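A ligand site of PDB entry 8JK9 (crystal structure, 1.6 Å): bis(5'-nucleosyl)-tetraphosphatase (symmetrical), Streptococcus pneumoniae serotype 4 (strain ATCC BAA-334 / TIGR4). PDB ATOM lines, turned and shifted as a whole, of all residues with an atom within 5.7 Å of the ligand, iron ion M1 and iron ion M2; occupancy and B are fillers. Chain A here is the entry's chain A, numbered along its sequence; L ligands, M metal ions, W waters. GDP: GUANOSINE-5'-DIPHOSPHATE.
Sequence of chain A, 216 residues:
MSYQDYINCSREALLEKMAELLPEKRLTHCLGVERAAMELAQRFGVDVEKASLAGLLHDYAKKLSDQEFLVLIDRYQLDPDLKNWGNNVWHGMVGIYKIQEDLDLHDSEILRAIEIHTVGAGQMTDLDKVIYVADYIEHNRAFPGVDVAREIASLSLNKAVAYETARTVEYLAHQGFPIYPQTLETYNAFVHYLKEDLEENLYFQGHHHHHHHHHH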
ATOM      1  N   ARG A  26      -1.320  22.668   2.609  1.00  0.00           N
ATOM      2  CA  ARG A  26      -0.658  22.407   3.883  1.00  0.00           C
ATOM      3  C   ARG A  26      -0.846  20.953   4.332  1.00  0.00           C
ATOM      4  O   ARG A  26       0.107  20.354   4.829  1.00  0.00           O
ATOM      5  CB  ARG A  26      -1.134  23.389   4.972  1.00  0.00           C
ATOM      6  CG  ARG A  26      -0.408  23.305   6.324  1.00  0.00           C
ATOM      7  CD  ARG A  26       1.097  23.502   6.228  1.00  0.00           C
ATOM      8  NE  ARG A  26       1.436  24.730   5.498  1.00  0.00           N
ATOM      9  CZ  ARG A  26       2.677  25.144   5.246  1.00  0.00           C
ATOM     10  NH1 ARG A  26       2.858  26.274   4.576  1.00  0.00           N
ATOM     11  NH2 ARG A  26       3.729  24.447   5.653  1.00  0.00           N
ATOM     12  N   HIS A  29       1.390  18.856   2.209  1.00  0.00           N
ATOM     13  CA  HIS A  29       2.732  18.989   2.764  1.00  0.00           C
ATOM     14  C   HIS A  29       2.925  18.061   3.967  1.00  0.00           C
ATOM     15  O   HIS A  29       3.904  17.327   4.010  1.00  0.00           O
ATOM     16  CB  HIS A  29       3.014  20.474   3.101  1.00  0.00           C
ATOM     17  CG  HIS A  29       4.174  20.681   4.031  1.00  0.00           C
ATOM     18  ND1 HIS A  29       5.476  20.462   3.642  1.00  0.00           N
ATOM     19  CD2 HIS A  29       4.228  21.110   5.317  1.00  0.00           C
ATOM     20  CE1 HIS A  29       6.283  20.728   4.658  1.00  0.00           C
ATOM     21  NE2 HIS A  29       5.552  21.130   5.678  1.00  0.00           N
ATOM     22  N   VAL A  33       5.655  15.100   4.484  1.00  0.00           N
ATOM     23  CA  VAL A  33       6.586  14.994   5.615  1.00  0.00           C
ATOM     24  C   VAL A  33       6.440  13.640   6.329  1.00  0.00           C
ATOM     25  O   VAL A  33       7.433  13.038   6.717  1.00  0.00           O
ATOM     26  CB  VAL A  33       6.435  16.208   6.575  1.00  0.00           C
ATOM     27  CG1 VAL A  33       7.400  16.116   7.757  1.00  0.00           C
ATOM     28  CG2 VAL A  33       6.698  17.492   5.823  1.00  0.00           C
ATOM     29  N   HIS A  58       3.492  17.727  12.315  1.00  0.00           N
ATOM     30  CA  HIS A  58       4.439  18.804  12.650  1.00  0.00           C
ATOM     31  C   HIS A  58       3.855  20.210  12.404  1.00  0.00           C
ATOM     32  O   HIS A  58       4.105  21.125  13.204  1.00  0.00           O
ATOM     33  CB  HIS A  58       5.776  18.625  11.924  1.00  0.00           C
ATOM     34  CG  HIS A  58       5.747  19.104  10.515  1.00  0.00           C
ATOM     35  ND1 HIS A  58       5.111  18.422   9.504  1.00  0.00           N
ATOM     36  CD2 HIS A  58       6.234  20.240   9.959  1.00  0.00           C
ATOM     37  CE1 HIS A  58       5.220  19.106   8.378  1.00  0.00           C
ATOM     38  NE2 HIS A  58       5.902  20.204   8.631  1.00  0.00           N
ATOM     39  N   ASP A  59       3.041  20.363  11.351  1.00  0.00           N
ATOM     40  CA  ASP A  59       2.416  21.645  11.020  1.00  0.00           C
ATOM     41  C   ASP A  59       0.921  21.731  11.375  1.00  0.00           C
ATOM     42  O   ASP A  59       0.201  22.587  10.837  1.00  0.00           O
ATOM     43  CB  ASP A  59       2.624  22.006   9.528  1.00  0.00           C
ATOM     44  CG  ASP A  59       3.962  22.688   9.258  1.00  0.00           C
ATOM     45  OD1 ASP A  59       4.616  23.205  10.194  1.00  0.00           O
ATOM     46  OD2 ASP A  59       4.367  22.683   8.074  1.00  0.00           O
ATOM     47  N   LYS A  62      -0.235  25.224  12.247  1.00  0.00           N
ATOM     48  CA  LYS A  62       0.220  26.275  11.327  1.00  0.00           C
ATOM     49  C   LYS A  62      -0.744  27.459  11.188  1.00  0.00           C
ATOM     50  O   LYS A  62      -0.312  28.601  10.971  1.00  0.00           O
ATOM     51  CB  LYS A  62       0.513  25.675   9.951  1.00  0.00           C
ATOM     52  CG  LYS A  62       1.126  26.619   8.935  1.00  0.00           C
ATOM     53  CD  LYS A  62       2.618  26.829   9.148  1.00  0.00           C
ATOM     54  CE  LYS A  62       3.256  27.525   7.966  1.00  0.00           C
ATOM     55  NZ  LYS A  62       4.717  27.754   8.209  1.00  0.00           N
ATOM     56  N   TRP A  85       7.679  37.348  19.010  1.00  0.00           N
ATOM     57  CA  TRP A  85       7.896  36.651  17.738  1.00  0.00           C
ATOM     58  C   TRP A  85       6.551  36.442  17.030  1.00  0.00           C
ATOM     59  O   TRP A  85       5.648  37.281  17.164  1.00  0.00           O
ATOM     60  CB  TRP A  85       8.732  35.370  17.968  1.00  0.00           C
ATOM     61  CG  TRP A  85      10.084  35.713  18.560  1.00  0.00           C
ATOM     62  CD1 TRP A  85      10.374  35.850  19.889  1.00  0.00           C
ATOM     63  CD2 TRP A  85      11.279  36.038  17.853  1.00  0.00           C
ATOM     64  NE1 TRP A  85      11.691  36.204  20.059  1.00  0.00           N
ATOM     65  CE2 TRP A  85      12.270  36.336  18.827  1.00  0.00           C
ATOM     66  CE3 TRP A  85      11.619  36.084  16.497  1.00  0.00           C
ATOM     67  CZ2 TRP A  85      13.577  36.682  18.476  1.00  0.00           C
ATOM     68  CZ3 TRP A  85      12.939  36.424  16.156  1.00  0.00           C
ATOM     69  CH2 TRP A  85      13.885  36.725  17.139  1.00  0.00           C
ATOM     70  N   ASN A  88       5.946  31.788  12.689  1.00  0.00           N
ATOM     71  CA  ASN A  88       7.130  30.980  12.359  1.00  0.00           C
ATOM     72  C   ASN A  88       7.724  30.259  13.566  1.00  0.00           C
ATOM     73  O   ASN A  88       7.939  29.051  13.530  1.00  0.00           O
ATOM     74  CB  ASN A  88       8.202  31.816  11.651  1.00  0.00           C
ATOM     75  CG  ASN A  88       7.798  32.207  10.232  1.00  0.00           C
ATOM     76  OD1 ASN A  88       6.773  31.770   9.712  1.00  0.00           O
ATOM     77  ND2 ASN A  88       8.633  33.032   9.593  1.00  0.00           N
ATOM     78  N   VAL A  89       7.936  31.015  14.649  1.00  0.00           N
ATOM     79  CA  VAL A  89       8.423  30.445  15.906  1.00  0.00           C
ATOM     80  C   VAL A  89       7.297  29.683  16.624  1.00  0.00           C
ATOM     81  O   VAL A  89       7.516  28.579  17.112  1.00  0.00           O
ATOM     82  CB  VAL A  89       9.032  31.550  16.818  1.00  0.00           C
ATOM     83  CG1 VAL A  89       9.416  30.978  18.180  1.00  0.00           C
ATOM     84  CG2 VAL A  89      10.260  32.158  16.160  1.00  0.00           C
ATOM     85  N   HIS A  91       4.343  28.113  15.764  1.00  0.00           N
ATOM     86  CA  HIS A  91       3.500  26.983  15.332  1.00  0.00           C
ATOM     87  C   HIS A  91       4.033  25.640  15.817  1.00  0.00           C
ATOM     88  O   HIS A  91       3.247  24.741  16.126  1.00  0.00           O
ATOM     89  CB  HIS A  91       3.121  27.006  13.843  1.00  0.00           C
ATOM     90  CG  HIS A  91       4.228  26.627  12.901  1.00  0.00           C
ATOM     91  ND1 HIS A  91       5.278  27.461  12.612  1.00  0.00           N
ATOM     92  CD2 HIS A  91       4.417  25.502  12.175  1.00  0.00           C
ATOM     93  CE1 HIS A  91       6.091  26.863  11.750  1.00  0.00           C
ATOM     94  NE2 HIS A  91       5.587  25.676  11.472  1.00  0.00           N
ATOM     95  N   HIS A 117      10.797  21.751  15.287  1.00  0.00           N
ATOM     96  CA  HIS A 117      10.909  21.413  13.850  1.00  0.00           C
ATOM     97  C   HIS A 117      11.320  22.596  12.952  1.00  0.00           C
ATOM     98  O   HIS A 117      11.858  22.385  11.869  1.00  0.00           O
ATOM     99  CB  HIS A 117       9.644  20.748  13.303  1.00  0.00           C
ATOM    100  CG  HIS A 117       8.581  21.711  12.873  1.00  0.00           C
ATOM    101  ND1 HIS A 117       7.551  22.101  13.709  1.00  0.00           N
ATOM    102  CD2 HIS A 117       8.380  22.366  11.701  1.00  0.00           C
ATOM    103  CE1 HIS A 117       6.762  22.952  13.077  1.00  0.00           C
ATOM    104  NE2 HIS A 117       7.250  23.122  11.852  1.00  0.00           N
ATOM    105  N   THR A 118      11.015  23.807  13.395  1.00  0.00           N
ATOM    106  CA  THR A 118      11.319  24.999  12.592  1.00  0.00           C
ATOM    107  C   THR A 118      12.733  25.522  12.882  1.00  0.00           C
ATOM    108  O   THR A 118      13.507  25.796  11.954  1.00  0.00           O
ATOM    109  CB  THR A 118      10.316  26.142  12.861  1.00  0.00           C
ATOM    110  OG1 THR A 118       8.973  25.668  12.686  1.00  0.00           O
ATOM    111  CG2 THR A 118      10.576  27.349  11.977  1.00  0.00           C
ATOM    112  N   VAL A 119      13.051  25.650  14.172  1.00  0.00           N
ATOM    113  CA  VAL A 119      14.267  26.317  14.617  1.00  0.00           C
ATOM    114  C   VAL A 119      15.413  25.367  15.002  1.00  0.00           C
ATOM    115  O   VAL A 119      16.569  25.786  15.056  1.00  0.00           O
ATOM    116  CB  VAL A 119      13.965  27.315  15.775  1.00  0.00           C
ATOM    117  CG1 VAL A 119      13.003  28.385  15.292  1.00  0.00           C
ATOM    118  CG2 VAL A 119      13.405  26.607  17.010  1.00  0.00           C
ATOM    119  N   ASP A 135      10.839  17.764   6.790  1.00  0.00           N
ATOM    120  CA  ASP A 135      10.075  18.956   6.500  1.00  0.00           C
ATOM    121  C   ASP A 135      10.615  19.710   5.275  1.00  0.00           C
ATOM    122  O   ASP A 135       9.863  20.210   4.444  1.00  0.00           O
ATOM    123  CB  ASP A 135      10.106  19.842   7.739  1.00  0.00           C
ATOM    124  CG  ASP A 135       9.243  21.067   7.616  1.00  0.00           C
ATOM    125  OD1 ASP A 135       8.196  21.023   6.936  1.00  0.00           O
ATOM    126  OD2 ASP A 135       9.616  22.078   8.233  1.00  0.00           O
ATOM    127  N   ARG A 141       8.017  19.858  -1.999  1.00  0.00           N
ATOM    128  CA  ARG A 141       8.884  21.035  -1.945  1.00  0.00           C
ATOM    129  C   ARG A 141       9.598  21.245  -3.259  1.00  0.00           C
ATOM    130  O   ARG A 141      10.119  20.297  -3.864  1.00  0.00           O
ATOM    131  CB  ARG A 141       9.915  20.948  -0.809  1.00  0.00           C
ATOM    132  CG  ARG A 141       9.360  20.943   0.607  1.00  0.00           C
ATOM    133  CD  ARG A 141       9.027  22.347   1.104  1.00  0.00           C
ATOM    134  NE  ARG A 141       9.118  22.422   2.563  1.00  0.00           N
ATOM    135  CZ  ARG A 141       8.302  23.116   3.347  1.00  0.00           C
ATOM    136  NH1 ARG A 141       8.491  23.104   4.668  1.00  0.00           N
ATOM    137  NH2 ARG A 141       7.295  23.822   2.842  1.00  0.00           N
ATOM    138  N   GLU A 164      20.497  22.579   5.886  1.00  0.00           N
ATOM    139  CA  GLU A 164      19.224  23.287   6.039  1.00  0.00           C
ATOM    140  C   GLU A 164      19.356  24.532   6.933  1.00  0.00           C
ATOM    141  O   GLU A 164      18.865  25.621   6.573  1.00  0.00           O
ATOM    142  CB  GLU A 164      18.139  22.350   6.564  1.00  0.00           C
ATOM    143  CG  GLU A 164      16.835  23.088   6.857  1.00  0.00           C
ATOM    144  CD  GLU A 164      15.718  22.202   7.371  1.00  0.00           C
ATOM    145  OE1 GLU A 164      15.897  20.967   7.423  1.00  0.00           O
ATOM    146  OE2 GLU A 164      14.664  22.771   7.721  1.00  0.00           O
ATOM    147  N   THR A 168      18.877  28.369   5.793  1.00  0.00           N
ATOM    148  CA  THR A 168      17.817  29.148   6.449  1.00  0.00           C
ATOM    149  C   THR A 168      18.339  30.459   7.042  1.00  0.00           C
ATOM    150  O   THR A 168      17.757  31.519   6.796  1.00  0.00           O
ATOM    151  CB  THR A 168      17.084  28.285   7.472  1.00  0.00           C
ATOM    152  OG1 THR A 168      16.443  27.230   6.741  1.00  0.00           O
ATOM    153  CG2 THR A 168      16.005  29.099   8.198  1.00  0.00           C
ATOM    154  N   LEU A 172      17.257  34.125   5.759  1.00  0.00           N
ATOM    155  CA  LEU A 172      16.648  35.087   6.681  1.00  0.00           C
ATOM    156  C   LEU A 172      17.392  36.420   6.633  1.00  0.00           C
ATOM    157  O   LEU A 172      16.754  37.488   6.556  1.00  0.00           O
ATOM    158  CB  LEU A 172      16.593  34.519   8.104  1.00  0.00           C
ATOM    159  CG  LEU A 172      15.613  33.369   8.316  1.00  0.00           C
ATOM    160  CD1 LEU A 172      15.955  32.695   9.633  1.00  0.00           C
ATOM    161  CD2 LEU A 172      14.160  33.833   8.264  1.00  0.00           C
ATOM    162  N   PHE A 177      14.919  39.413   7.811  1.00  0.00           N
ATOM    163  CA  PHE A 177      14.010  38.975   8.869  1.00  0.00           C
ATOM    164  C   PHE A 177      14.756  38.640  10.155  1.00  0.00           C
ATOM    165  O   PHE A 177      15.878  38.128  10.090  1.00  0.00           O
ATOM    166  CB  PHE A 177      13.239  37.723   8.427  1.00  0.00           C
ATOM    167  CG  PHE A 177      12.391  37.907   7.182  1.00  0.00           C
ATOM    168  CD1 PHE A 177      11.815  39.144   6.872  1.00  0.00           C
ATOM    169  CD2 PHE A 177      12.147  36.822   6.348  1.00  0.00           C
ATOM    170  CE1 PHE A 177      11.022  39.285   5.729  1.00  0.00           C
ATOM    171  CE2 PHE A 177      11.344  36.959   5.214  1.00  0.00           C
ATOM    172  CZ  PHE A 177      10.795  38.185   4.905  1.00  0.00           C
ATOM    173  N   PRO A 178      14.146  38.907  11.327  1.00  0.00           N
ATOM    174  CA  PRO A 178      14.797  38.565  12.608  1.00  0.00           C
ATOM    175  C   PRO A 178      15.069  37.065  12.736  1.00  0.00           C
ATOM    176  O   PRO A 178      14.251  36.269  12.295  1.00  0.00           O
ATOM    177  CB  PRO A 178      13.779  39.000  13.676  1.00  0.00           C
ATOM    178  CG  PRO A 178      12.752  39.808  12.973  1.00  0.00           C
ATOM    179  CD  PRO A 178      12.832  39.554  11.507  1.00  0.00           C
ATOM    180  N   ILE A 179      16.206  36.714  13.338  1.00  0.00           N
ATOM    181  CA  ILE A 179      16.620  35.315  13.466  1.00  0.00           C
ATOM    182  C   ILE A 179      16.444  34.935  14.929  1.00  0.00           C
ATOM    183  O   ILE A 179      17.057  35.534  15.806  1.00  0.00           O
ATOM    184  CB  ILE A 179      18.080  35.119  12.996  1.00  0.00           C
ATOM    185  CG1 ILE A 179      18.174  35.390  11.496  1.00  0.00           C
ATOM    186  CG2 ILE A 179      18.602  33.719  13.338  1.00  0.00           C
ATOM    187  CD1 ILE A 179      19.573  35.667  10.986  1.00  0.00           C
ATOM    188  N   TYR A 180      15.608  33.930  15.162  1.00  0.00           N
ATOM    189  CA  TYR A 180      15.361  33.446  16.519  1.00  0.00           C
ATOM    190  C   TYR A 180      16.650  32.931  17.163  1.00  0.00           C
ATOM    191  O   TYR A 180      17.398  32.196  16.524  1.00  0.00           O
ATOM    192  CB  TYR A 180      14.273  32.352  16.497  1.00  0.00           C
ATOM    193  CG  TYR A 180      13.724  32.025  17.855  1.00  0.00           C
ATOM    194  CD1 TYR A 180      13.092  33.012  18.617  1.00  0.00           C
ATOM    195  CD2 TYR A 180      13.793  30.729  18.361  1.00  0.00           C
ATOM    196  CE1 TYR A 180      12.571  32.708  19.876  1.00  0.00           C
ATOM    197  CE2 TYR A 180      13.275  30.417  19.620  1.00  0.00           C
ATOM    198  CZ  TYR A 180      12.667  31.402  20.363  1.00  0.00           C
ATOM    199  OH  TYR A 180      12.161  31.062  21.602  1.00  0.00           O
ATOM    200  N   THR A 183      17.537  29.300  16.675  1.00  0.00           N
ATOM    201  CA  THR A 183      18.020  29.027  15.307  1.00  0.00           C
ATOM    202  C   THR A 183      19.549  29.136  15.219  1.00  0.00           C
ATOM    203  O   THR A 183      20.211  28.291  14.613  1.00  0.00           O
ATOM    204  CB  THR A 183      17.326  29.964  14.292  1.00  0.00           C
ATOM    205  OG1 THR A 183      15.918  29.699  14.321  1.00  0.00           O
ATOM    206  CG2 THR A 183      17.842  29.748  12.867  1.00  0.00           C
HETATM  207  PB  GDP L   1       6.803  25.163   7.135  1.00  0.00           P
HETATM  208  O1B GDP L   1       6.620  23.831   6.437  1.00  0.00           O
HETATM  209  O2B GDP L   1       6.663  26.326   6.172  1.00  0.00           O
HETATM  210  O3B GDP L   1       5.984  25.321   8.405  1.00  0.00           O
HETATM  211  O3A GDP L   1       8.379  25.200   7.498  1.00  0.00           O
HETATM  212  PA  GDP L   1       9.113  25.648   8.866  1.00  0.00           P
HETATM  213  O1A GDP L   1       8.244  25.408  10.072  1.00  0.00           O
HETATM  214  O2A GDP L   1      10.506  25.074   8.873  1.00  0.00           O
HETATM  215  O5' GDP L   1       9.330  27.231   8.683  1.00  0.00           O
HETATM  216  C5' GDP L   1       8.310  28.187   8.504  1.00  0.00           C
HETATM  217  C4' GDP L   1       8.963  29.539   8.213  1.00  0.00           C
HETATM  218  O4' GDP L   1       9.699  29.904   9.389  1.00  0.00           O
HETATM  219  C3' GDP L   1       9.944  29.555   7.036  1.00  0.00           C
HETATM  220  O3' GDP L   1       9.653  30.677   6.175  1.00  0.00           O
HETATM  221  C2' GDP L   1      11.300  29.693   7.702  1.00  0.00           C
HETATM  222  O2' GDP L   1      12.303  30.340   6.915  1.00  0.00           O
HETATM  223  C1' GDP L   1      10.915  30.483   8.950  1.00  0.00           C
HETATM  224  N9  GDP L   1      11.961  30.534   9.990  1.00  0.00           N
HETATM  225  C8  GDP L   1      12.770  29.532  10.388  1.00  0.00           C
HETATM  226  N7  GDP L   1      13.619  29.967  11.350  1.00  0.00           N
HETATM  227  C5  GDP L   1      13.346  31.269  11.537  1.00  0.00           C
HETATM  228  C6  GDP L   1      13.852  32.343  12.392  1.00  0.00           C
HETATM  229  O6  GDP L   1      14.785  32.123  13.169  1.00  0.00           O
HETATM  230  N1  GDP L   1      13.295  33.564  12.263  1.00  0.00           N
HETATM  231  C2  GDP L   1      12.283  33.828  11.404  1.00  0.00           C
HETATM  232  N2  GDP L   1      11.774  35.080  11.337  1.00  0.00           N
HETATM  233  N3  GDP L   1      11.743  32.881  10.600  1.00  0.00           N
HETATM  234  C4  GDP L   1      12.244  31.626  10.646  1.00  0.00           C
HETATM  235 FE    FE M   1       6.315  21.976   7.460  1.00  0.00          FE
HETATM  236 FE    FE M   2       6.432  24.242  10.186  1.00  0.00          FE
HETATM  237 MG    MG M   3       7.811  26.572  14.984  1.00  0.00          MG
HETATM  238  O   HOH W   1      11.062  23.603   6.090  1.00  0.00           O
HETATM  239  O   HOH W   2       7.169  22.925   8.999  1.00  0.00           O
HETATM  240  O   HOH W   3       5.715  26.180   3.731  1.00  0.00           O
HETATM  241  O   HOH W   4       5.661  29.486   5.789  1.00  0.00           O
HETATM  242  O   HOH W   5      12.789  26.353   9.184  1.00  0.00           O
HETATM  243  O   HOH W   6      15.439  27.740  11.377  1.00  0.00           O
HETATM  244  O   HOH W   7       9.059  26.853   4.413  1.00  0.00           O
HETATM  245  O   HOH W   8      12.180  22.666   9.148  1.00  0.00           O
HETATM  246  O   HOH W   9      10.901  33.711   6.891  1.00  0.00           O
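O2B of the ligand is in salt-bridge range of NH1 of Arg 141 (3.998 Å).
OG1 of Thr 118 sits close to O1A of the ligand, at 2.7 Å.
O2B of the ligand lies within salt-bridge range of NZ of Lys 62 (3.2 Å).
O6 of the ligand lies within hydrogen-bond range of N of Tyr 180.
A nitrogen (N1) of the ligand sits at hydrogen-bond distance from the backbone carbonyl oxygen (O) of Pro 178, at 2.9 Å.
O6 of the ligand lies within hydrogen-bond range of OG1 of Thr 183 (2.9 Å).
The guanidinium group of Arg 26 lies within salt-bridge range of an oxygen (O2B) of the ligand, at 3.5 Å.
N3 of the ligand sits at hydrogen-bond distance from ND2 of Asn 88.
The side-chain carboxylate (OD2) of Asp 59 sits close to the guanidinium group (NH2) of Arg 26 (3.1 Å).
ND1 of His 91 lies within hydrogen-bond range of O of Asn 88, 3.2 Å away.
A ring nitrogen (NE2) of His 117 lies close to the side-chain hydroxyl (OG1) of Thr 118 (3.2 Å).
The guanidinium group (NH1) of Arg 141 is in salt-bridge range of the side-chain carboxylate (OD2) of Asp 135.
The backbone carbonyl oxygen (O) of Leu 172 is in hydrogen-bond range of the backbone NH (N) of Phe 177.
The side-chain hydroxyl (OG1) of Thr 168 lies within hydrogen-bond range of the backbone carbonyl oxygen (O) of Glu 164, at 2.9 Å.
Merely in contact with the ligand: Leu 172, Ile 179 and Thr 168.
Within 4 Å of the ligand: Arg 26, His 29, Asp 59, Lys 62, Asn 88, His 91, His 117, Thr 118, Asp 135, Arg 141, Thr 168, Leu 172, Pro 178, Ile 179, Tyr 180 and Thr 183.
The nearest printed residue that does not touch the ligand is Phe 177 (4.2 Å).
Residues that only touch iron ion M1: Arg 141 (3.7 Å).
Of the 23 residues printed, 5 come within 4 Å of iron ion M1.
Thr 118 touches iron ion M2 (OG1 to FE, 3.8 Å).
The nearest printed residue that does not touch iron ion M2 is His 58 (4.01 Å).
Iron ion M1 is bound by water W2, NE2 of His 29, O1B of the ligand, OD2 of Asp 59, NE2 of His 58 and OD1 of Asp 135.
Iron ion M1 has six donor atoms within binding distance.
Water W2 is bound to iron ion M2.
OD1 of Asp 59 is bound to iron ion M2 (2.1 Å).
NE2 of His 91 binds iron ion M2, 2.1 Å away.
Iron ion M2 is bound by an oxygen (O3B) of the ligand, 2.1 Å away.
O1A of the ligand is bound to iron ion M2 (2.2 Å).
Iron ion M2 is bound by a ring nitrogen (NE2) of His 117 (2.2 Å).
Iron ion M2 has six donor atoms within binding distance.
Water W2 lies within hydrogen-bond range of OD2 of Asp 135 (2.7 Å) and O3A of the ligand (3.0 Å).
Water W3 lies within hydrogen-bond range of an oxygen (O2B) of the ligand (2.6 Å), the guanidinium group (NH2) of Arg 141 (3.0 Å) and the guanidinium group (NH1) of Arg 26 (3.0 Å).
Water W5 bridges an oxygen (O2A) of the ligand (2.6 Å) and the backbone carbonyl oxygen of Thr 118 (2.9 Å).
Water W6 lies within hydrogen-bond range of the backbone carbonyl oxygen of Thr 118 (2.8 Å) and a nitrogen (N7) of the ligand (2.9 Å).
Water W1 lies within hydrogen-bond range of NH1 of Arg 141 (3.0 Å), OD2 of Asp 135 (3.0 Å) and O2A of the ligand (3.2 Å).
Water W4 lies within hydrogen-bond range of NZ of Lys 62 (3.1 Å) and O2B of the ligand (3.3 Å).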
